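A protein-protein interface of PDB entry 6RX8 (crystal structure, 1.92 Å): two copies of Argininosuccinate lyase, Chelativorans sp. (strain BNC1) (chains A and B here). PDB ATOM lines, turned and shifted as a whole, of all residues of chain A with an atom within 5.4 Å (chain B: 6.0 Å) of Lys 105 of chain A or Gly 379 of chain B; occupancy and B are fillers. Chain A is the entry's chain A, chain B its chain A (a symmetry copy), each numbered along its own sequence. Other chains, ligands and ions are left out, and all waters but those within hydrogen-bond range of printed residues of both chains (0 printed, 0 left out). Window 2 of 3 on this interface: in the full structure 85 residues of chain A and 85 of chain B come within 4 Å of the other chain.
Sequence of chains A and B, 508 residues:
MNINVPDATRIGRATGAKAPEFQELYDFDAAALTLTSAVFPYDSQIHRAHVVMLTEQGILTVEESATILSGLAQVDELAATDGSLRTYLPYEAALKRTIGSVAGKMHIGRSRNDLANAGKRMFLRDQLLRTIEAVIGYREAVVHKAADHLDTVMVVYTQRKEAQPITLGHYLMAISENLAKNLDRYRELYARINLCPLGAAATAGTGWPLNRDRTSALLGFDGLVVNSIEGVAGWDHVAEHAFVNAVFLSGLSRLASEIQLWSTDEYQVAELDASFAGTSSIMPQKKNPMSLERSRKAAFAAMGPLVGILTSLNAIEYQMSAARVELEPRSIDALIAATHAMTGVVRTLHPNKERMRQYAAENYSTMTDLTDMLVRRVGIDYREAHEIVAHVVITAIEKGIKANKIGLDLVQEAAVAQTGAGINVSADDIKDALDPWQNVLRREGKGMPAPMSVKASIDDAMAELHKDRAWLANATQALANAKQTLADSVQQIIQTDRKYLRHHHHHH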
ATOM      1  N   LEU A  54      17.383   9.811 -16.999  1.00  0.00           N
ATOM      2  CA  LEU A  54      16.233   9.882 -16.106  1.00  0.00           C
ATOM      3  C   LEU A  54      14.944  10.111 -16.893  1.00  0.00           C
ATOM      4  O   LEU A  54      13.880   9.600 -16.525  1.00  0.00           O
ATOM      5  CB  LEU A  54      16.417  10.995 -15.074  1.00  0.00           C
ATOM      6  CG  LEU A  54      17.554  10.895 -14.059  1.00  0.00           C
ATOM      7  CD1 LEU A  54      17.611  12.194 -13.245  1.00  0.00           C
ATOM      8  CD2 LEU A  54      17.401   9.694 -13.143  1.00  0.00           C
ATOM      9  N   LEU A  60      12.063  11.663 -14.702  1.00  0.00           N
ATOM     10  CA  LEU A  60      11.704  13.038 -15.003  1.00  0.00           C
ATOM     11  C   LEU A  60      10.734  13.053 -16.175  1.00  0.00           C
ATOM     12  O   LEU A  60      10.884  12.268 -17.118  1.00  0.00           O
ATOM     13  CB  LEU A  60      12.917  13.882 -15.381  1.00  0.00           C
ATOM     14  CG  LEU A  60      14.098  13.985 -14.426  1.00  0.00           C
ATOM     15  CD1 LEU A  60      15.241  14.713 -15.133  1.00  0.00           C
ATOM     16  CD2 LEU A  60      13.709  14.698 -13.155  1.00  0.00           C
ATOM     17  N   GLU A  64       9.993  18.639 -17.177  1.00  0.00           N
ATOM     18  CA  GLU A  64      11.037  18.848 -16.177  1.00  0.00           C
ATOM     19  C   GLU A  64      12.423  18.763 -16.805  1.00  0.00           C
ATOM     20  O   GLU A  64      13.296  19.592 -16.527  1.00  0.00           O
ATOM     21  CB  GLU A  64      10.912  17.813 -15.060  1.00  0.00           C
ATOM     22  CG  GLU A  64       9.654  17.935 -14.236  1.00  0.00           C
ATOM     23  CD  GLU A  64       9.514  16.807 -13.233  1.00  0.00           C
ATOM     24  OE1 GLU A  64       9.896  15.664 -13.562  1.00  0.00           O
ATOM     25  OE2 GLU A  64       9.029  17.067 -12.114  1.00  0.00           O
ATOM     26  N   ILE A  68      15.354  21.707 -16.895  1.00  0.00           N
ATOM     27  CA  ILE A  68      16.698  21.495 -16.363  1.00  0.00           C
ATOM     28  C   ILE A  68      17.735  21.675 -17.461  1.00  0.00           C
ATOM     29  O   ILE A  68      18.727  22.393 -17.289  1.00  0.00           O
ATOM     30  CB  ILE A  68      16.800  20.095 -15.730  1.00  0.00           C
ATOM     31  CG1 ILE A  68      15.912  20.016 -14.488  1.00  0.00           C
ATOM     32  CG2 ILE A  68      18.245  19.731 -15.387  1.00  0.00           C
ATOM     33  CD1 ILE A  68      15.553  18.592 -14.107  1.00  0.00           C
ATOM     34  N   SER A 101      13.129  25.080  -8.165  1.00  0.00           N
ATOM     35  CA  SER A 101      13.459  23.914  -7.357  1.00  0.00           C
ATOM     36  C   SER A 101      13.605  22.639  -8.177  1.00  0.00           C
ATOM     37  O   SER A 101      14.256  21.699  -7.710  1.00  0.00           O
ATOM     38  CB  SER A 101      12.398  23.716  -6.275  1.00  0.00           C
ATOM     39  OG  SER A 101      11.126  23.493  -6.853  1.00  0.00           O
ATOM     40  N   VAL A 102      13.021  22.579  -9.379  1.00  0.00           N
ATOM     41  CA  VAL A 102      13.176  21.403 -10.230  1.00  0.00           C
ATOM     42  C   VAL A 102      14.651  21.122 -10.505  1.00  0.00           C
ATOM     43  O   VAL A 102      15.019  19.991 -10.842  1.00  0.00           O
ATOM     44  CB  VAL A 102      12.385  21.583 -11.545  1.00  0.00           C
ATOM     45  CG1 VAL A 102      13.052  22.626 -12.443  1.00  0.00           C
ATOM     46  CG2 VAL A 102      12.236  20.245 -12.267  1.00  0.00           C
ATOM     47  N   ALA A 103      15.512  22.133 -10.355  1.00  0.00           N
ATOM     48  CA  ALA A 103      16.947  21.920 -10.490  1.00  0.00           C
ATOM     49  C   ALA A 103      17.420  20.741  -9.647  1.00  0.00           C
ATOM     50  O   ALA A 103      18.276  19.962 -10.081  1.00  0.00           O
ATOM     51  CB  ALA A 103      17.697  23.190 -10.089  1.00  0.00           C
ATOM     52  N   GLY A 104      16.881  20.601  -8.434  1.00  0.00           N
ATOM     53  CA  GLY A 104      17.327  19.552  -7.535  1.00  0.00           C
ATOM     54  C   GLY A 104      17.083  18.156  -8.056  1.00  0.00           C
ATOM     55  O   GLY A 104      17.768  17.214  -7.644  1.00  0.00           O
ATOM     56  N   LYS A 105      16.137  17.997  -8.974  1.00  0.00           N
ATOM     57  CA  LYS A 105      15.816  16.664  -9.451  1.00  0.00           C
ATOM     58  C   LYS A 105      16.914  16.090 -10.328  1.00  0.00           C
ATOM     59  O   LYS A 105      16.931  14.880 -10.563  1.00  0.00           O
ATOM     60  CB  LYS A 105      14.496  16.675 -10.209  1.00  0.00           C
ATOM     61  CG  LYS A 105      13.300  16.927  -9.328  1.00  0.00           C
ATOM     62  CD  LYS A 105      12.022  16.472 -10.016  1.00  0.00           C
ATOM     63  CE  LYS A 105      10.838  16.596  -9.088  1.00  0.00           C
ATOM     64  NZ  LYS A 105       9.599  16.054  -9.711  1.00  0.00           N
ATOM     65  N   MET A 106      17.837  16.913 -10.816  1.00  0.00           N
ATOM     66  CA  MET A 106      18.875  16.335 -11.653  1.00  0.00           C
ATOM     67  C   MET A 106      19.812  15.428 -10.861  1.00  0.00           C
ATOM     68  O   MET A 106      20.589  14.691 -11.468  1.00  0.00           O
ATOM     69  CB  MET A 106      19.671  17.436 -12.356  1.00  0.00           C
ATOM     70  CG  MET A 106      20.663  18.179 -11.483  1.00  0.00           C
ATOM     71  SD  MET A 106      22.072  18.772 -12.450  1.00  0.00           S
ATOM     72  CE  MET A 106      22.780  19.973 -11.337  1.00  0.00           C
ATOM     73  N   HIS A 107      19.765  15.463  -9.534  1.00  0.00           N
ATOM     74  CA  HIS A 107      20.657  14.653  -8.713  1.00  0.00           C
ATOM     75  C   HIS A 107      20.012  13.358  -8.249  1.00  0.00           C
ATOM     76  O   HIS A 107      20.629  12.612  -7.475  1.00  0.00           O
ATOM     77  CB  HIS A 107      21.111  15.455  -7.501  1.00  0.00           C
ATOM     78  CG  HIS A 107      22.464  15.072  -6.989  1.00  0.00           C
ATOM     79  ND1 HIS A 107      23.536  14.830  -7.820  1.00  0.00           N
ATOM     80  CD2 HIS A 107      22.928  14.926  -5.726  1.00  0.00           C
ATOM     81  CE1 HIS A 107      24.600  14.545  -7.092  1.00  0.00           C
ATOM     82  NE2 HIS A 107      24.259  14.604  -5.817  1.00  0.00           N
ATOM     83  N   ILE A 108      18.775  13.094  -8.676  1.00  0.00           N
ATOM     84  CA  ILE A 108      18.086  11.873  -8.289  1.00  0.00           C
ATOM     85  C   ILE A 108      18.940  10.676  -8.678  1.00  0.00           C
ATOM     86  O   ILE A 108      19.396  10.562  -9.823  1.00  0.00           O
ATOM     87  CB  ILE A 108      16.694  11.819  -8.942  1.00  0.00           C
ATOM     88  CG1 ILE A 108      15.752  12.838  -8.285  1.00  0.00           C
ATOM     89  CG2 ILE A 108      16.110  10.394  -8.886  1.00  0.00           C
ATOM     90  CD1 ILE A 108      14.484  13.109  -9.095  1.00  0.00           C
ATOM     91  N   LEU B 374      10.696  10.498   0.045  1.00  0.00           N
ATOM     92  CA  LEU B 374       9.988  11.774   0.027  1.00  0.00           C
ATOM     93  C   LEU B 374       9.894  12.328  -1.389  1.00  0.00           C
ATOM     94  O   LEU B 374       8.860  12.880  -1.786  1.00  0.00           O
ATOM     95  CB  LEU B 374      10.686  12.791   0.929  1.00  0.00           C
ATOM     96  CG  LEU B 374      10.811  12.426   2.408  1.00  0.00           C
ATOM     97  CD1 LEU B 374      11.436  13.581   3.189  1.00  0.00           C
ATOM     98  CD2 LEU B 374       9.464  12.023   2.994  1.00  0.00           C
ATOM     99  N   VAL B 375      10.977  12.215  -2.156  1.00  0.00           N
ATOM    100  CA  VAL B 375      10.965  12.651  -3.548  1.00  0.00           C
ATOM    101  C   VAL B 375       9.987  11.810  -4.354  1.00  0.00           C
ATOM    102  O   VAL B 375       9.158  12.333  -5.104  1.00  0.00           O
ATOM    103  CB  VAL B 375      12.385  12.567  -4.135  1.00  0.00           C
ATOM    104  CG1 VAL B 375      12.385  12.898  -5.613  1.00  0.00           C
ATOM    105  CG2 VAL B 375      13.308  13.488  -3.373  1.00  0.00           C
ATOM    106  N   ARG B 376      10.098  10.488  -4.231  1.00  0.00           N
ATOM    107  CA  ARG B 376       9.258   9.582  -5.004  1.00  0.00           C
ATOM    108  C   ARG B 376       7.796   9.737  -4.622  1.00  0.00           C
ATOM    109  O   ARG B 376       6.913   9.716  -5.487  1.00  0.00           O
ATOM    110  CB  ARG B 376       9.743   8.146  -4.786  1.00  0.00           C
ATOM    111  CG  ARG B 376       8.913   7.053  -5.441  1.00  0.00           C
ATOM    112  CD  ARG B 376       9.466   5.654  -5.095  1.00  0.00           C
ATOM    113  NE  ARG B 376      10.876   5.507  -5.467  1.00  0.00           N
ATOM    114  CZ  ARG B 376      11.901   5.482  -4.612  1.00  0.00           C
ATOM    115  NH1 ARG B 376      11.698   5.581  -3.303  1.00  0.00           N
ATOM    116  NH2 ARG B 376      13.140   5.354  -5.072  1.00  0.00           N
ATOM    117  N   ARG B 377       7.521   9.946  -3.336  1.00  0.00           N
ATOM    118  CA  ARG B 377       6.146   9.948  -2.855  1.00  0.00           C
ATOM    119  C   ARG B 377       5.460  11.305  -3.004  1.00  0.00           C
ATOM    120  O   ARG B 377       4.336  11.373  -3.507  1.00  0.00           O
ATOM    121  CB  ARG B 377       6.111   9.496  -1.392  1.00  0.00           C
ATOM    122  CG  ARG B 377       4.789   8.877  -0.985  1.00  0.00           C
ATOM    123  CD  ARG B 377       4.643   7.489  -1.587  1.00  0.00           C
ATOM    124  NE  ARG B 377       5.450   6.510  -0.866  1.00  0.00           N
ATOM    125  CZ  ARG B 377       6.018   5.441  -1.419  1.00  0.00           C
ATOM    126  NH1 ARG B 377       5.888   5.204  -2.720  1.00  0.00           N
ATOM    127  NH2 ARG B 377       6.731   4.613  -0.665  1.00  0.00           N
ATOM    128  N   VAL B 378       6.090  12.394  -2.570  1.00  0.00           N
ATOM    129  CA  VAL B 378       5.427  13.695  -2.607  1.00  0.00           C
ATOM    130  C   VAL B 378       5.964  14.591  -3.710  1.00  0.00           C
ATOM    131  O   VAL B 378       5.439  15.699  -3.904  1.00  0.00           O
ATOM    132  CB  VAL B 378       5.499  14.411  -1.244  1.00  0.00           C
ATOM    133  CG1 VAL B 378       5.389  13.402  -0.114  1.00  0.00           C
ATOM    134  CG2 VAL B 378       6.765  15.221  -1.113  1.00  0.00           C
ATOM    135  N   GLY B 379       6.992  14.154  -4.432  1.00  0.00           N
ATOM    136  CA  GLY B 379       7.440  14.854  -5.615  1.00  0.00           C
ATOM    137  C   GLY B 379       8.297  16.071  -5.378  1.00  0.00           C
ATOM    138  O   GLY B 379       8.616  16.772  -6.345  1.00  0.00           O
ATOM    139  N   ILE B 380       8.674  16.362  -4.126  1.00  0.00           N
ATOM    140  CA  ILE B 380       9.608  17.459  -3.887  1.00  0.00           C
ATOM    141  C   ILE B 380      10.956  17.102  -4.514  1.00  0.00           C
ATOM    142  O   ILE B 380      11.257  15.933  -4.788  1.00  0.00           O
ATOM    143  CB  ILE B 380       9.775  17.782  -2.395  1.00  0.00           C
ATOM    144  CG1 ILE B 380      10.275  16.562  -1.620  1.00  0.00           C
ATOM    145  CG2 ILE B 380       8.465  18.291  -1.820  1.00  0.00           C
ATOM    146  CD1 ILE B 380      10.504  16.841  -0.136  1.00  0.00           C
ATOM    147  N   ASP B 381      11.776  18.127  -4.742  1.00  0.00           N
ATOM    148  CA  ASP B 381      13.093  17.908  -5.326  1.00  0.00           C
ATOM    149  C   ASP B 381      14.040  17.304  -4.290  1.00  0.00           C
ATOM    150  O   ASP B 381      13.788  17.342  -3.079  1.00  0.00           O
ATOM    151  CB  ASP B 381      13.676  19.213  -5.872  1.00  0.00           C
ATOM    152  CG  ASP B 381      14.014  20.206  -4.779  1.00  0.00           C
ATOM    153  OD1 ASP B 381      13.078  20.814  -4.213  1.00  0.00           O
ATOM    154  OD2 ASP B 381      15.220  20.362  -4.487  1.00  0.00           O
ATOM    155  N   TYR B 382      15.147  16.734  -4.783  1.00  0.00           N
ATOM    156  CA  TYR B 382      16.020  15.985  -3.888  1.00  0.00           C
ATOM    157  C   TYR B 382      16.640  16.904  -2.842  1.00  0.00           C
ATOM    158  O   TYR B 382      16.800  16.511  -1.682  1.00  0.00           O
ATOM    159  CB  TYR B 382      17.118  15.236  -4.651  1.00  0.00           C
ATOM    160  CG  TYR B 382      17.769  14.201  -3.747  1.00  0.00           C
ATOM    161  CD1 TYR B 382      17.162  12.972  -3.533  1.00  0.00           C
ATOM    162  CD2 TYR B 382      18.946  14.476  -3.057  1.00  0.00           C
ATOM    163  CE1 TYR B 382      17.709  12.031  -2.685  1.00  0.00           C
ATOM    164  CE2 TYR B 382      19.514  13.531  -2.200  1.00  0.00           C
ATOM    165  CZ  TYR B 382      18.881  12.306  -2.021  1.00  0.00           C
ATOM    166  OH  TYR B 382      19.395  11.344  -1.181  1.00  0.00           O
ATOM    167  N   ARG B 383      16.970  18.143  -3.221  1.00  0.00           N
ATOM    168  CA  ARG B 383      17.689  19.005  -2.288  1.00  0.00           C
ATOM    169  C   ARG B 383      16.809  19.396  -1.105  1.00  0.00           C
ATOM    170  O   ARG B 383      17.294  19.463   0.031  1.00  0.00           O
ATOM    171  CB  ARG B 383      18.229  20.242  -3.003  1.00  0.00           C
ATOM    172  CG  ARG B 383      19.174  21.100  -2.151  1.00  0.00           C
ATOM    173  CD  ARG B 383      20.359  20.293  -1.626  1.00  0.00           C
ATOM    174  NE  ARG B 383      21.039  19.601  -2.718  1.00  0.00           N
ATOM    175  CZ  ARG B 383      21.562  18.383  -2.634  1.00  0.00           C
ATOM    176  NH1 ARG B 383      21.505  17.699  -1.494  1.00  0.00           N
ATOM    177  NH2 ARG B 383      22.144  17.848  -3.704  1.00  0.00           N
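No position is printed for both chains.
Printed residues of chain B that touch a printed residue of chain A: Gly 379, Asp 381, Tyr 382 and Arg 383.
Hydrophobic or aromatic side chains of chain B within 4 Å of the printed part of chain A: Tyr 382.
Along chain A the printed residues that touch a printed residue of chain B span positions 101 to 107.
Among the printed residues, no Asp or Glu carboxylate lies within 4 Å of a Lys or Arg side-chain nitrogen of the other chain.
OE2 of Glu 64 of chain A is in salt-bridge range of NZ of Lys 105 of chain A (2.7 Å).
The backbone carbonyl oxygen of Leu 374 of chain B lies within hydrogen-bond range of the backbone NH of Gly 379 of chain B.
The backbone NH (N) of Arg 383 of chain B is in hydrogen-bond range of the side-chain carboxylate (OD2) of Asp 381 of chain B.
Lys 105 of chain A touches just one residue of chain B: Gly 379.
Of the printed residues of chain B, His 107 of chain A touches Arg 383 (3.6 Å).
Of chain A, only Lys 105 comes within 4 Å of Gly 379 of chain B.
Printed residues of chain A within 4 Å of Asp 381 of chain B: Ser 101 and Gly 104.
Of the printed residues of chain A, Tyr 382 of chain B touches Gly 104 (3.6 Å).
Printed residues of chain A within 4 Å of Arg 383 of chain B: His 107.
The nearest printed residue of chain A that does not touch Gly 379 of chain B is Glu 64 of chain A (5.8 Å).
CB of Asp 381 of chain B touches O of Ser 101 of chain A, 3.1 Å away.
CA of Gly 104 of chain A touches OD2 of Asp 381 of chain B, 3.8 Å away.
O of Gly 104 of chain A touches CB of Tyr 382 of chain B, at 3.6 Å.
CE of Lys 105 of chain A touches O of Gly 379 of chain B, at 3.5 Å.
His 107 of chain A touches Arg 383 of chain B.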
